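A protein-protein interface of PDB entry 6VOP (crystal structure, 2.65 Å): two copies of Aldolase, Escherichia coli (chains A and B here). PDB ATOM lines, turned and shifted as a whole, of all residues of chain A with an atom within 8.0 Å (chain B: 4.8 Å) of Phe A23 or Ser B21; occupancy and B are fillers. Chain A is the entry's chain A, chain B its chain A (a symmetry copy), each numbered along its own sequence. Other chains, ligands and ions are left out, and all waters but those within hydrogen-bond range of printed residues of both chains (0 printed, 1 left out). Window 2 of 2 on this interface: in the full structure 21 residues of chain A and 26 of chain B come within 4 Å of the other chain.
N of Gly A30 is in hydrogen-bond range of OE2 of Glu B182, at 2.9 Å.
The side-chain hydroxyl (OG) of Ser B21 lies within hydrogen-bond range of the guanidinium group (NE) of Arg B25, 3.0 Å away.
The side-chain carboxylate (OE2) of Glu B182 lies within salt-bridge range of the guanidinium group (NH1) of Arg B25, at 2.8 Å.
NE2 of Gln A24 is in hydrogen-bond range of OG of Ser A20, 2.9 Å away.
Among the printed residues, pairs that only touch across the chains: Phe A23 with Ser B21, Phe A23 with Arg B25, Phe A23 with Glu B182, Gln A24 with Arg B25, Thr A29 with Glu B182 and Asn A55 with Arg B17.
Phe A23 touches just these residues of chain B: Ser B21 (3.2 Å), Arg B25 (3.3 Å) and Glu B182 (3.95 Å).
Ser B21 touches just one residue of chain A: Phe A23 (3.2 Å).
Of the printed residues of chain B, Asn A55 touches Arg B17.
Of the printed residues of chain B, Thr A29 touches Glu B182.
Printed residues of chain B within 4 Å of Gly A30: Glu B182.
Printed residues of chain A within 4 Å of Glu B182: Phe A23 (3.95 Å), Thr A29 (3.9 Å) and Gly A30 (2.9 Å).
Printed residues of chain A within 4 Å of Arg B17: Asn A55 (3.4 Å).
The nearest printed residue of chain B that does not touch Phe A23 is Phe B22 (6.8 Å).
Of the 10 printed residues of chain B, 4 touch a printed residue of chain A.
Hydrophobic or aromatic side chains of chain A that line the printed part of chain B: Phe A23.
Among the printed residues, 7 pairs touch across the chains.
Among the printed residues, no Asp or Glu carboxylate lies within 4 Å of a Lys or Arg side-chain nitrogen of the other chain.
Phe A23 touches Ser B21, but with the chains exchanged Ser A21 does not touch Phe B23 (13.7 Å).
Phe A23 touches Arg B25, but with the chains exchanged Arg A25 does not touch Phe B23 (10.9 Å).
Gln A24 touches Arg B25, but with the chains exchanged Arg A25 does not touch Gln B24 (7.6 Å).
Of the 7 pairs that touch across the chains among the printed residues, none has its exchanged pair printed and touching as well.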
ATOM      1  N   THR A  16     -19.956 -17.643   8.072  1.00  0.00           N
ATOM      2  CA  THR A  16     -18.880 -18.305   7.343  1.00  0.00           C
ATOM      3  C   THR A  16     -17.602 -17.476   7.376  1.00  0.00           C
ATOM      4  O   THR A  16     -16.510 -18.013   7.605  1.00  0.00           O
ATOM      5  CB  THR A  16     -19.313 -18.559   5.897  1.00  0.00           C
ATOM      6  OG1 THR A  16     -20.450 -19.430   5.884  1.00  0.00           O
ATOM      7  CG2 THR A  16     -18.186 -19.193   5.100  1.00  0.00           C
ATOM      8  N   ARG A  17     -17.720 -16.163   7.157  1.00  0.00           N
ATOM      9  CA  ARG A  17     -16.543 -15.301   7.129  1.00  0.00           C
ATOM     10  C   ARG A  17     -15.878 -15.234   8.498  1.00  0.00           C
ATOM     11  O   ARG A  17     -14.655 -15.385   8.616  1.00  0.00           O
ATOM     12  CB  ARG A  17     -16.937 -13.902   6.643  1.00  0.00           C
ATOM     13  CG  ARG A  17     -15.768 -12.964   6.377  1.00  0.00           C
ATOM     14  CD  ARG A  17     -15.689 -11.867   7.428  1.00  0.00           C
ATOM     15  NE  ARG A  17     -16.906 -11.063   7.472  1.00  0.00           N
ATOM     16  CZ  ARG A  17     -17.140 -10.112   8.371  1.00  0.00           C
ATOM     17  NH1 ARG A  17     -16.239  -9.846   9.307  1.00  0.00           N
ATOM     18  NH2 ARG A  17     -18.277  -9.430   8.336  1.00  0.00           N
ATOM     19  N   ILE A  18     -16.672 -15.016   9.549  1.00  0.00           N
ATOM     20  CA  ILE A  18     -16.121 -14.925  10.898  1.00  0.00           C
ATOM     21  C   ILE A  18     -15.526 -16.262  11.329  1.00  0.00           C
ATOM     22  O   ILE A  18     -14.477 -16.306  11.985  1.00  0.00           O
ATOM     23  CB  ILE A  18     -17.209 -14.436  11.875  1.00  0.00           C
ATOM     24  CG1 ILE A  18     -17.464 -12.941  11.675  1.00  0.00           C
ATOM     25  CG2 ILE A  18     -16.819 -14.722  13.316  1.00  0.00           C
ATOM     26  CD1 ILE A  18     -18.348 -12.330  12.735  1.00  0.00           C
ATOM     27  N   ALA A  19     -16.174 -17.370  10.959  1.00  0.00           N
ATOM     28  CA  ALA A  19     -15.645 -18.686  11.305  1.00  0.00           C
ATOM     29  C   ALA A  19     -14.278 -18.912  10.674  1.00  0.00           C
ATOM     30  O   ALA A  19     -13.349 -19.395  11.333  1.00  0.00           O
ATOM     31  CB  ALA A  19     -16.623 -19.778  10.874  1.00  0.00           C
ATOM     32  N   SER A  20     -14.140 -18.564   9.392  1.00  0.00           N
ATOM     33  CA  SER A  20     -12.858 -18.729   8.717  1.00  0.00           C
ATOM     34  C   SER A  20     -11.777 -17.888   9.385  1.00  0.00           C
ATOM     35  O   SER A  20     -10.633 -18.334   9.534  1.00  0.00           O
ATOM     36  CB  SER A  20     -13.003 -18.362   7.241  1.00  0.00           C
ATOM     37  OG  SER A  20     -11.743 -18.298   6.602  1.00  0.00           O
ATOM     38  N   SER A  21     -12.122 -16.670   9.804  1.00  0.00           N
ATOM     39  CA  SER A  21     -11.160 -15.815  10.493  1.00  0.00           C
ATOM     40  C   SER A  21     -10.640 -16.473  11.766  1.00  0.00           C
ATOM     41  O   SER A  21      -9.433 -16.462  12.029  1.00  0.00           O
ATOM     42  CB  SER A  21     -11.804 -14.464  10.806  1.00  0.00           C
ATOM     43  OG  SER A  21     -10.856 -13.566  11.343  1.00  0.00           O
ATOM     44  N   PHE A  22     -11.539 -17.049  12.569  1.00  0.00           N
ATOM     45  CA  PHE A  22     -11.112 -17.753  13.774  1.00  0.00           C
ATOM     46  C   PHE A  22     -10.183 -18.911  13.436  1.00  0.00           C
ATOM     47  O   PHE A  22      -9.217 -19.176  14.160  1.00  0.00           O
ATOM     48  CB  PHE A  22     -12.330 -18.259  14.543  1.00  0.00           C
ATOM     49  CG  PHE A  22     -13.005 -17.208  15.370  1.00  0.00           C
ATOM     50  CD1 PHE A  22     -12.262 -16.269  16.067  1.00  0.00           C
ATOM     51  CD2 PHE A  22     -14.387 -17.161  15.454  1.00  0.00           C
ATOM     52  CE1 PHE A  22     -12.886 -15.299  16.830  1.00  0.00           C
ATOM     53  CE2 PHE A  22     -15.016 -16.196  16.214  1.00  0.00           C
ATOM     54  CZ  PHE A  22     -14.264 -15.263  16.903  1.00  0.00           C
ATOM     55  N   PHE A  23     -10.457 -19.608  12.333  1.00  0.00           N
ATOM     56  CA  PHE A  23      -9.674 -20.787  11.984  1.00  0.00           C
ATOM     57  C   PHE A  23      -8.279 -20.408  11.498  1.00  0.00           C
ATOM     58  O   PHE A  23      -7.286 -21.016  11.915  1.00  0.00           O
ATOM     59  CB  PHE A  23     -10.420 -21.603  10.929  1.00  0.00           C
ATOM     60  CG  PHE A  23      -9.709 -22.859  10.505  1.00  0.00           C
ATOM     61  CD1 PHE A  23      -9.843 -24.028  11.235  1.00  0.00           C
ATOM     62  CD2 PHE A  23      -8.926 -22.875   9.363  1.00  0.00           C
ATOM     63  CE1 PHE A  23      -9.195 -25.185  10.840  1.00  0.00           C
ATOM     64  CE2 PHE A  23      -8.280 -24.026   8.967  1.00  0.00           C
ATOM     65  CZ  PHE A  23      -8.416 -25.181   9.704  1.00  0.00           C
ATOM     66  N   GLN A  24      -8.183 -19.399  10.622  1.00  0.00           N
ATOM     67  CA  GLN A  24      -6.885 -19.033  10.058  1.00  0.00           C
ATOM     68  C   GLN A  24      -5.975 -18.381  11.093  1.00  0.00           C
ATOM     69  O   GLN A  24      -4.748 -18.438  10.956  1.00  0.00           O
ATOM     70  CB  GLN A  24      -7.067 -18.105   8.853  1.00  0.00           C
ATOM     71  CG  GLN A  24      -8.056 -18.616   7.809  1.00  0.00           C
ATOM     72  CD  GLN A  24      -8.337 -17.599   6.711  1.00  0.00           C
ATOM     73  OE1 GLN A  24      -7.682 -17.597   5.668  1.00  0.00           O
ATOM     74  NE2 GLN A  24      -9.314 -16.729   6.945  1.00  0.00           N
ATOM     75  N   ARG A  25      -6.542 -17.769  12.129  1.00  0.00           N
ATOM     76  CA  ARG A  25      -5.758 -17.065  13.132  1.00  0.00           C
ATOM     77  C   ARG A  25      -5.486 -17.909  14.371  1.00  0.00           C
ATOM     78  O   ARG A  25      -4.928 -17.396  15.346  1.00  0.00           O
ATOM     79  CB  ARG A  25      -6.456 -15.760  13.523  1.00  0.00           C
ATOM     80  CG  ARG A  25      -6.570 -14.760  12.382  1.00  0.00           C
ATOM     81  CD  ARG A  25      -7.231 -13.480  12.854  1.00  0.00           C
ATOM     82  NE  ARG A  25      -8.576 -13.732  13.361  1.00  0.00           N
ATOM     83  CZ  ARG A  25      -9.137 -13.056  14.357  1.00  0.00           C
ATOM     84  NH1 ARG A  25      -8.469 -12.082  14.959  1.00  0.00           N
ATOM     85  NH2 ARG A  25     -10.368 -13.354  14.749  1.00  0.00           N
ATOM     86  N   GLY A  26      -5.859 -19.186  14.353  1.00  0.00           N
ATOM     87  CA  GLY A  26      -5.508 -20.104  15.415  1.00  0.00           C
ATOM     88  C   GLY A  26      -6.475 -20.169  16.577  1.00  0.00           C
ATOM     89  O   GLY A  26      -6.176 -20.852  17.567  1.00  0.00           O
ATOM     90  N   TYR A  27      -7.618 -19.486  16.499  1.00  0.00           N
ATOM     91  CA  TYR A  27      -8.585 -19.546  17.591  1.00  0.00           C
ATOM     92  C   TYR A  27      -9.329 -20.877  17.602  1.00  0.00           C
ATOM     93  O   TYR A  27      -9.651 -21.405  18.671  1.00  0.00           O
ATOM     94  CB  TYR A  27      -9.577 -18.390  17.485  1.00  0.00           C
ATOM     95  CG  TYR A  27      -9.004 -17.029  17.807  1.00  0.00           C
ATOM     96  CD1 TYR A  27      -8.481 -16.220  16.806  1.00  0.00           C
ATOM     97  CD2 TYR A  27      -9.002 -16.544  19.109  1.00  0.00           C
ATOM     98  CE1 TYR A  27      -7.963 -14.971  17.095  1.00  0.00           C
ATOM     99  CE2 TYR A  27      -8.486 -15.295  19.408  1.00  0.00           C
ATOM    100  CZ  TYR A  27      -7.969 -14.513  18.398  1.00  0.00           C
ATOM    101  OH  TYR A  27      -7.458 -13.270  18.687  1.00  0.00           O
ATOM    102  N   ALA A  28      -9.624 -21.424  16.426  1.00  0.00           N
ATOM    103  CA  ALA A  28     -10.341 -22.685  16.295  1.00  0.00           C
ATOM    104  C   ALA A  28      -9.375 -23.790  15.891  1.00  0.00           C
ATOM    105  O   ALA A  28      -8.517 -23.588  15.028  1.00  0.00           O
ATOM    106  CB  ALA A  28     -11.464 -22.568  15.264  1.00  0.00           C
ATOM    107  N   THR A  29      -9.517 -24.957  16.516  1.00  0.00           N
ATOM    108  CA  THR A  29      -8.604 -26.084  16.315  1.00  0.00           C
ATOM    109  C   THR A  29      -9.398 -27.285  15.812  1.00  0.00           C
ATOM    110  O   THR A  29     -10.119 -27.928  16.583  1.00  0.00           O
ATOM    111  CB  THR A  29      -7.862 -26.427  17.603  1.00  0.00           C
ATOM    112  OG1 THR A  29      -8.746 -26.282  18.722  1.00  0.00           O
ATOM    113  CG2 THR A  29      -6.665 -25.512  17.787  1.00  0.00           C
ATOM    114  N   GLY A  30      -9.247 -27.594  14.527  1.00  0.00           N
ATOM    115  CA  GLY A  30      -9.963 -28.726  13.950  1.00  0.00           C
ATOM    116  C   GLY A  30     -11.464 -28.486  13.907  1.00  0.00           C
ATOM    117  O   GLY A  30     -11.935 -27.387  13.585  1.00  0.00           O
ATOM    118  N   SER A  31     -12.227 -29.540  14.217  1.00  0.00           N
ATOM    119  CA  SER A  31     -13.683 -29.505  14.343  1.00  0.00           C
ATOM    120  C   SER A  31     -14.142 -29.133  15.745  1.00  0.00           C
ATOM    121  O   SER A  31     -15.308 -29.361  16.092  1.00  0.00           O
ATOM    122  CB  SER A  31     -14.273 -30.862  13.964  1.00  0.00           C
ATOM    123  OG  SER A  31     -14.303 -31.718  15.087  1.00  0.00           O
ATOM    124  N   ALA A  32     -13.252 -28.599  16.571  1.00  0.00           N
ATOM    125  CA  ALA A  32     -13.592 -28.246  17.946  1.00  0.00           C
ATOM    126  C   ALA A  32     -14.145 -26.823  17.969  1.00  0.00           C
ATOM    127  O   ALA A  32     -13.392 -25.848  17.888  1.00  0.00           O
ATOM    128  CB  ALA A  32     -12.367 -28.406  18.837  1.00  0.00           C
ATOM    129  N   SER A  51     -18.026 -30.180  11.253  1.00  0.00           N
ATOM    130  CA  SER A  51     -17.735 -29.172  10.246  1.00  0.00           C
ATOM    131  C   SER A  51     -16.493 -28.393  10.654  1.00  0.00           C
ATOM    132  O   SER A  51     -16.413 -27.883  11.777  1.00  0.00           O
ATOM    133  CB  SER A  51     -18.926 -28.229  10.058  1.00  0.00           C
ATOM    134  OG  SER A  51     -18.996 -27.770   8.720  1.00  0.00           O
ATOM    135  N   CYS A  52     -15.528 -28.316   9.742  1.00  0.00           N
ATOM    136  CA  CYS A  52     -14.331 -27.514   9.952  1.00  0.00           C
ATOM    137  C   CYS A  52     -14.679 -26.041   9.763  1.00  0.00           C
ATOM    138  O   CYS A  52     -15.171 -25.647   8.700  1.00  0.00           O
ATOM    139  CB  CYS A  52     -13.229 -27.945   8.987  1.00  0.00           C
ATOM    140  SG  CYS A  52     -11.788 -26.859   8.955  1.00  0.00           S
ATOM    141  N   LEU A  53     -14.418 -25.231  10.791  1.00  0.00           N
ATOM    142  CA  LEU A  53     -14.815 -23.828  10.758  1.00  0.00           C
ATOM    143  C   LEU A  53     -14.119 -23.044   9.649  1.00  0.00           C
ATOM    144  O   LEU A  53     -14.603 -21.970   9.268  1.00  0.00           O
ATOM    145  CB  LEU A  53     -14.537 -23.179  12.115  1.00  0.00           C
ATOM    146  CG  LEU A  53     -15.466 -23.593  13.257  1.00  0.00           C
ATOM    147  CD1 LEU A  53     -15.202 -22.750  14.496  1.00  0.00           C
ATOM    148  CD2 LEU A  53     -16.924 -23.487  12.835  1.00  0.00           C
ATOM    149  N   GLY A  54     -13.008 -23.553   9.116  1.00  0.00           N
ATOM    150  CA  GLY A  54     -12.280 -22.845   8.079  1.00  0.00           C
ATOM    151  C   GLY A  54     -12.817 -23.009   6.672  1.00  0.00           C
ATOM    152  O   GLY A  54     -12.390 -22.275   5.775  1.00  0.00           O
ATOM    153  N   ASN A  55     -13.740 -23.946   6.455  1.00  0.00           N
ATOM    154  CA  ASN A  55     -14.298 -24.202   5.132  1.00  0.00           C
ATOM    155  C   ASN A  55     -15.785 -24.538   5.261  1.00  0.00           C
ATOM    156  O   ASN A  55     -16.250 -25.615   4.898  1.00  0.00           O
ATOM    157  CB  ASN A  55     -13.531 -25.321   4.427  1.00  0.00           C
ATOM    158  CG  ASN A  55     -13.929 -25.474   2.973  1.00  0.00           C
ATOM    159  OD1 ASN A  55     -14.482 -24.554   2.370  1.00  0.00           O
ATOM    160  ND2 ASN A  55     -13.651 -26.640   2.401  1.00  0.00           N
ATOM    161  N   LEU A  99     -15.453 -21.659  21.286  1.00  0.00           N
ATOM    162  CA  LEU A  99     -14.218 -22.189  20.735  1.00  0.00           C
ATOM    163  C   LEU A  99     -13.377 -22.778  21.859  1.00  0.00           C
ATOM    164  O   LEU A  99     -13.571 -22.462  23.034  1.00  0.00           O
ATOM    165  CB  LEU A  99     -13.416 -21.107  19.998  1.00  0.00           C
ATOM    166  CG  LEU A  99     -14.110 -20.384  18.843  1.00  0.00           C
ATOM    167  CD1 LEU A  99     -13.195 -19.324  18.259  1.00  0.00           C
ATOM    168  CD2 LEU A  99     -14.528 -21.377  17.775  1.00  0.00           C
ATOM    169  N   ARG B  17      -5.456 -28.579  -0.420  1.00  0.00           N
ATOM    170  CA  ARG B  17      -6.085 -27.557   0.411  1.00  0.00           C
ATOM    171  C   ARG B  17      -5.710 -27.735   1.878  1.00  0.00           C
ATOM    172  O   ARG B  17      -5.327 -26.772   2.555  1.00  0.00           O
ATOM    173  CB  ARG B  17      -7.605 -27.599   0.225  1.00  0.00           C
ATOM    174  CG  ARG B  17      -8.362 -26.455   0.883  1.00  0.00           C
ATOM    175  CD  ARG B  17      -9.149 -26.934   2.092  1.00  0.00           C
ATOM    176  NE  ARG B  17     -10.119 -27.967   1.740  1.00  0.00           N
ATOM    177  CZ  ARG B  17     -10.857 -28.631   2.624  1.00  0.00           C
ATOM    178  NH1 ARG B  17     -10.734 -28.373   3.919  1.00  0.00           N
ATOM    179  NH2 ARG B  17     -11.714 -29.557   2.213  1.00  0.00           N
ATOM    180  N   ILE B  18      -5.808 -28.966   2.384  1.00  0.00           N
ATOM    181  CA  ILE B  18      -5.482 -29.229   3.782  1.00  0.00           C
ATOM    182  C   ILE B  18      -3.999 -28.986   4.045  1.00  0.00           C
ATOM    183  O   ILE B  18      -3.620 -28.458   5.100  1.00  0.00           O
ATOM    184  CB  ILE B  18      -5.907 -30.662   4.159  1.00  0.00           C
ATOM    185  CG1 ILE B  18      -7.428 -30.742   4.303  1.00  0.00           C
ATOM    186  CG2 ILE B  18      -5.226 -31.118   5.439  1.00  0.00           C
ATOM    187  CD1 ILE B  18      -7.915 -32.046   4.885  1.00  0.00           C
ATOM    188  N   ALA B  19      -3.139 -29.352   3.091  1.00  0.00           N
ATOM    189  CA  ALA B  19      -1.707 -29.120   3.258  1.00  0.00           C
ATOM    190  C   ALA B  19      -1.403 -27.633   3.381  1.00  0.00           C
ATOM    191  O   ALA B  19      -0.625 -27.215   4.248  1.00  0.00           O
ATOM    192  CB  ALA B  19      -0.934 -29.730   2.090  1.00  0.00           C
ATOM    193  N   SER B  20      -2.015 -26.818   2.517  1.00  0.00           N
ATOM    194  CA  SER B  20      -1.794 -25.378   2.579  1.00  0.00           C
ATOM    195  C   SER B  20      -2.254 -24.812   3.918  1.00  0.00           C
ATOM    196  O   SER B  20      -1.595 -23.939   4.493  1.00  0.00           O
ATOM    197  CB  SER B  20      -2.519 -24.696   1.420  1.00  0.00           C
ATOM    198  OG  SER B  20      -2.513 -23.290   1.567  1.00  0.00           O
ATOM    199  N   SER B  21      -3.379 -25.306   4.436  1.00  0.00           N
ATOM    200  CA  SER B  21      -3.868 -24.852   5.734  1.00  0.00           C
ATOM    201  C   SER B  21      -2.849 -25.114   6.837  1.00  0.00           C
ATOM    202  O   SER B  21      -2.588 -24.240   7.670  1.00  0.00           O
ATOM    203  CB  SER B  21      -5.198 -25.537   6.052  1.00  0.00           C
ATOM    204  OG  SER B  21      -5.766 -25.012   7.233  1.00  0.00           O
ATOM    205  N   PHE B  22      -2.265 -26.315   6.857  1.00  0.00           N
ATOM    206  CA  PHE B  22      -1.233 -26.619   7.844  1.00  0.00           C
ATOM    207  C   PHE B  22      -0.045 -25.677   7.708  1.00  0.00           C
ATOM    208  O   PHE B  22       0.547 -25.260   8.711  1.00  0.00           O
ATOM    209  CB  PHE B  22      -0.778 -28.069   7.695  1.00  0.00           C
ATOM    210  CG  PHE B  22      -1.704 -29.064   8.324  1.00  0.00           C
ATOM    211  CD1 PHE B  22      -2.310 -28.797   9.542  1.00  0.00           C
ATOM    212  CD2 PHE B  22      -1.969 -30.271   7.699  1.00  0.00           C
ATOM    213  CE1 PHE B  22      -3.165 -29.715  10.123  1.00  0.00           C
ATOM    214  CE2 PHE B  22      -2.821 -31.192   8.273  1.00  0.00           C
ATOM    215  CZ  PHE B  22      -3.421 -30.914   9.487  1.00  0.00           C
ATOM    216  N   PHE B  23       0.314 -25.325   6.474  1.00  0.00           N
ATOM    217  CA  PHE B  23       1.495 -24.500   6.248  1.00  0.00           C
ATOM    218  C   PHE B  23       1.259 -23.057   6.679  1.00  0.00           C
ATOM    219  O   PHE B  23       2.111 -22.458   7.347  1.00  0.00           O
ATOM    220  CB  PHE B  23       1.897 -24.575   4.775  1.00  0.00           C
ATOM    221  CG  PHE B  23       3.122 -23.771   4.430  1.00  0.00           C
ATOM    222  CD1 PHE B  23       4.389 -24.300   4.610  1.00  0.00           C
ATOM    223  CD2 PHE B  23       3.003 -22.496   3.904  1.00  0.00           C
ATOM    224  CE1 PHE B  23       5.514 -23.564   4.285  1.00  0.00           C
ATOM    225  CE2 PHE B  23       4.122 -21.761   3.578  1.00  0.00           C
ATOM    226  CZ  PHE B  23       5.377 -22.295   3.767  1.00  0.00           C
ATOM    227  N   GLN B  24       0.104 -22.484   6.316  1.00  0.00           N
ATOM    228  CA  GLN B  24      -0.154 -21.081   6.630  1.00  0.00           C
ATOM    229  C   GLN B  24      -0.376 -20.861   8.123  1.00  0.00           C
ATOM    230  O   GLN B  24      -0.143 -19.756   8.624  1.00  0.00           O
ATOM    231  CB  GLN B  24      -1.357 -20.565   5.834  1.00  0.00           C
ATOM    232  CG  GLN B  24      -1.286 -20.844   4.336  1.00  0.00           C
ATOM    233  CD  GLN B  24      -2.566 -20.468   3.602  1.00  0.00           C
ATOM    234  OE1 GLN B  24      -2.701 -19.354   3.094  1.00  0.00           O
ATOM    235  NE2 GLN B  24      -3.513 -21.401   3.545  1.00  0.00           N
ATOM    236  N   ARG B  25      -0.815 -21.886   8.848  1.00  0.00           N
ATOM    237  CA  ARG B  25      -1.117 -21.754  10.266  1.00  0.00           C
ATOM    238  C   ARG B  25       0.030 -22.209  11.160  1.00  0.00           C
ATOM    239  O   ARG B  25      -0.134 -22.257  12.383  1.00  0.00           O
ATOM    240  CB  ARG B  25      -2.392 -22.528  10.605  1.00  0.00           C
ATOM    241  CG  ARG B  25      -3.638 -21.988   9.917  1.00  0.00           C
ATOM    242  CD  ARG B  25      -4.865 -22.775  10.334  1.00  0.00           C
ATOM    243  NE  ARG B  25      -4.737 -24.185   9.982  1.00  0.00           N
ATOM    244  CZ  ARG B  25      -5.245 -25.183  10.697  1.00  0.00           C
ATOM    245  NH1 ARG B  25      -5.919 -24.927  11.810  1.00  0.00           N
ATOM    246  NH2 ARG B  25      -5.081 -26.436  10.297  1.00  0.00           N
ATOM    247  N   GLU B 182      -4.556 -31.830  14.847  1.00  0.00           N
ATOM    248  CA  GLU B 182      -4.686 -30.493  15.411  1.00  0.00           C
ATOM    249  C   GLU B 182      -4.995 -30.535  16.904  1.00  0.00           C
ATOM    250  O   GLU B 182      -4.516 -29.676  17.653  1.00  0.00           O
ATOM    251  CB  GLU B 182      -5.755 -29.710  14.651  1.00  0.00           C
ATOM    252  CG  GLU B 182      -5.295 -29.234  13.277  1.00  0.00           C
ATOM    253  CD  GLU B 182      -6.352 -28.427  12.546  1.00  0.00           C
ATOM    254  OE1 GLU B 182      -6.811 -28.875  11.472  1.00  0.00           O
ATOM    255  OE2 GLU B 182      -6.721 -27.343  13.044  1.00  0.00           O
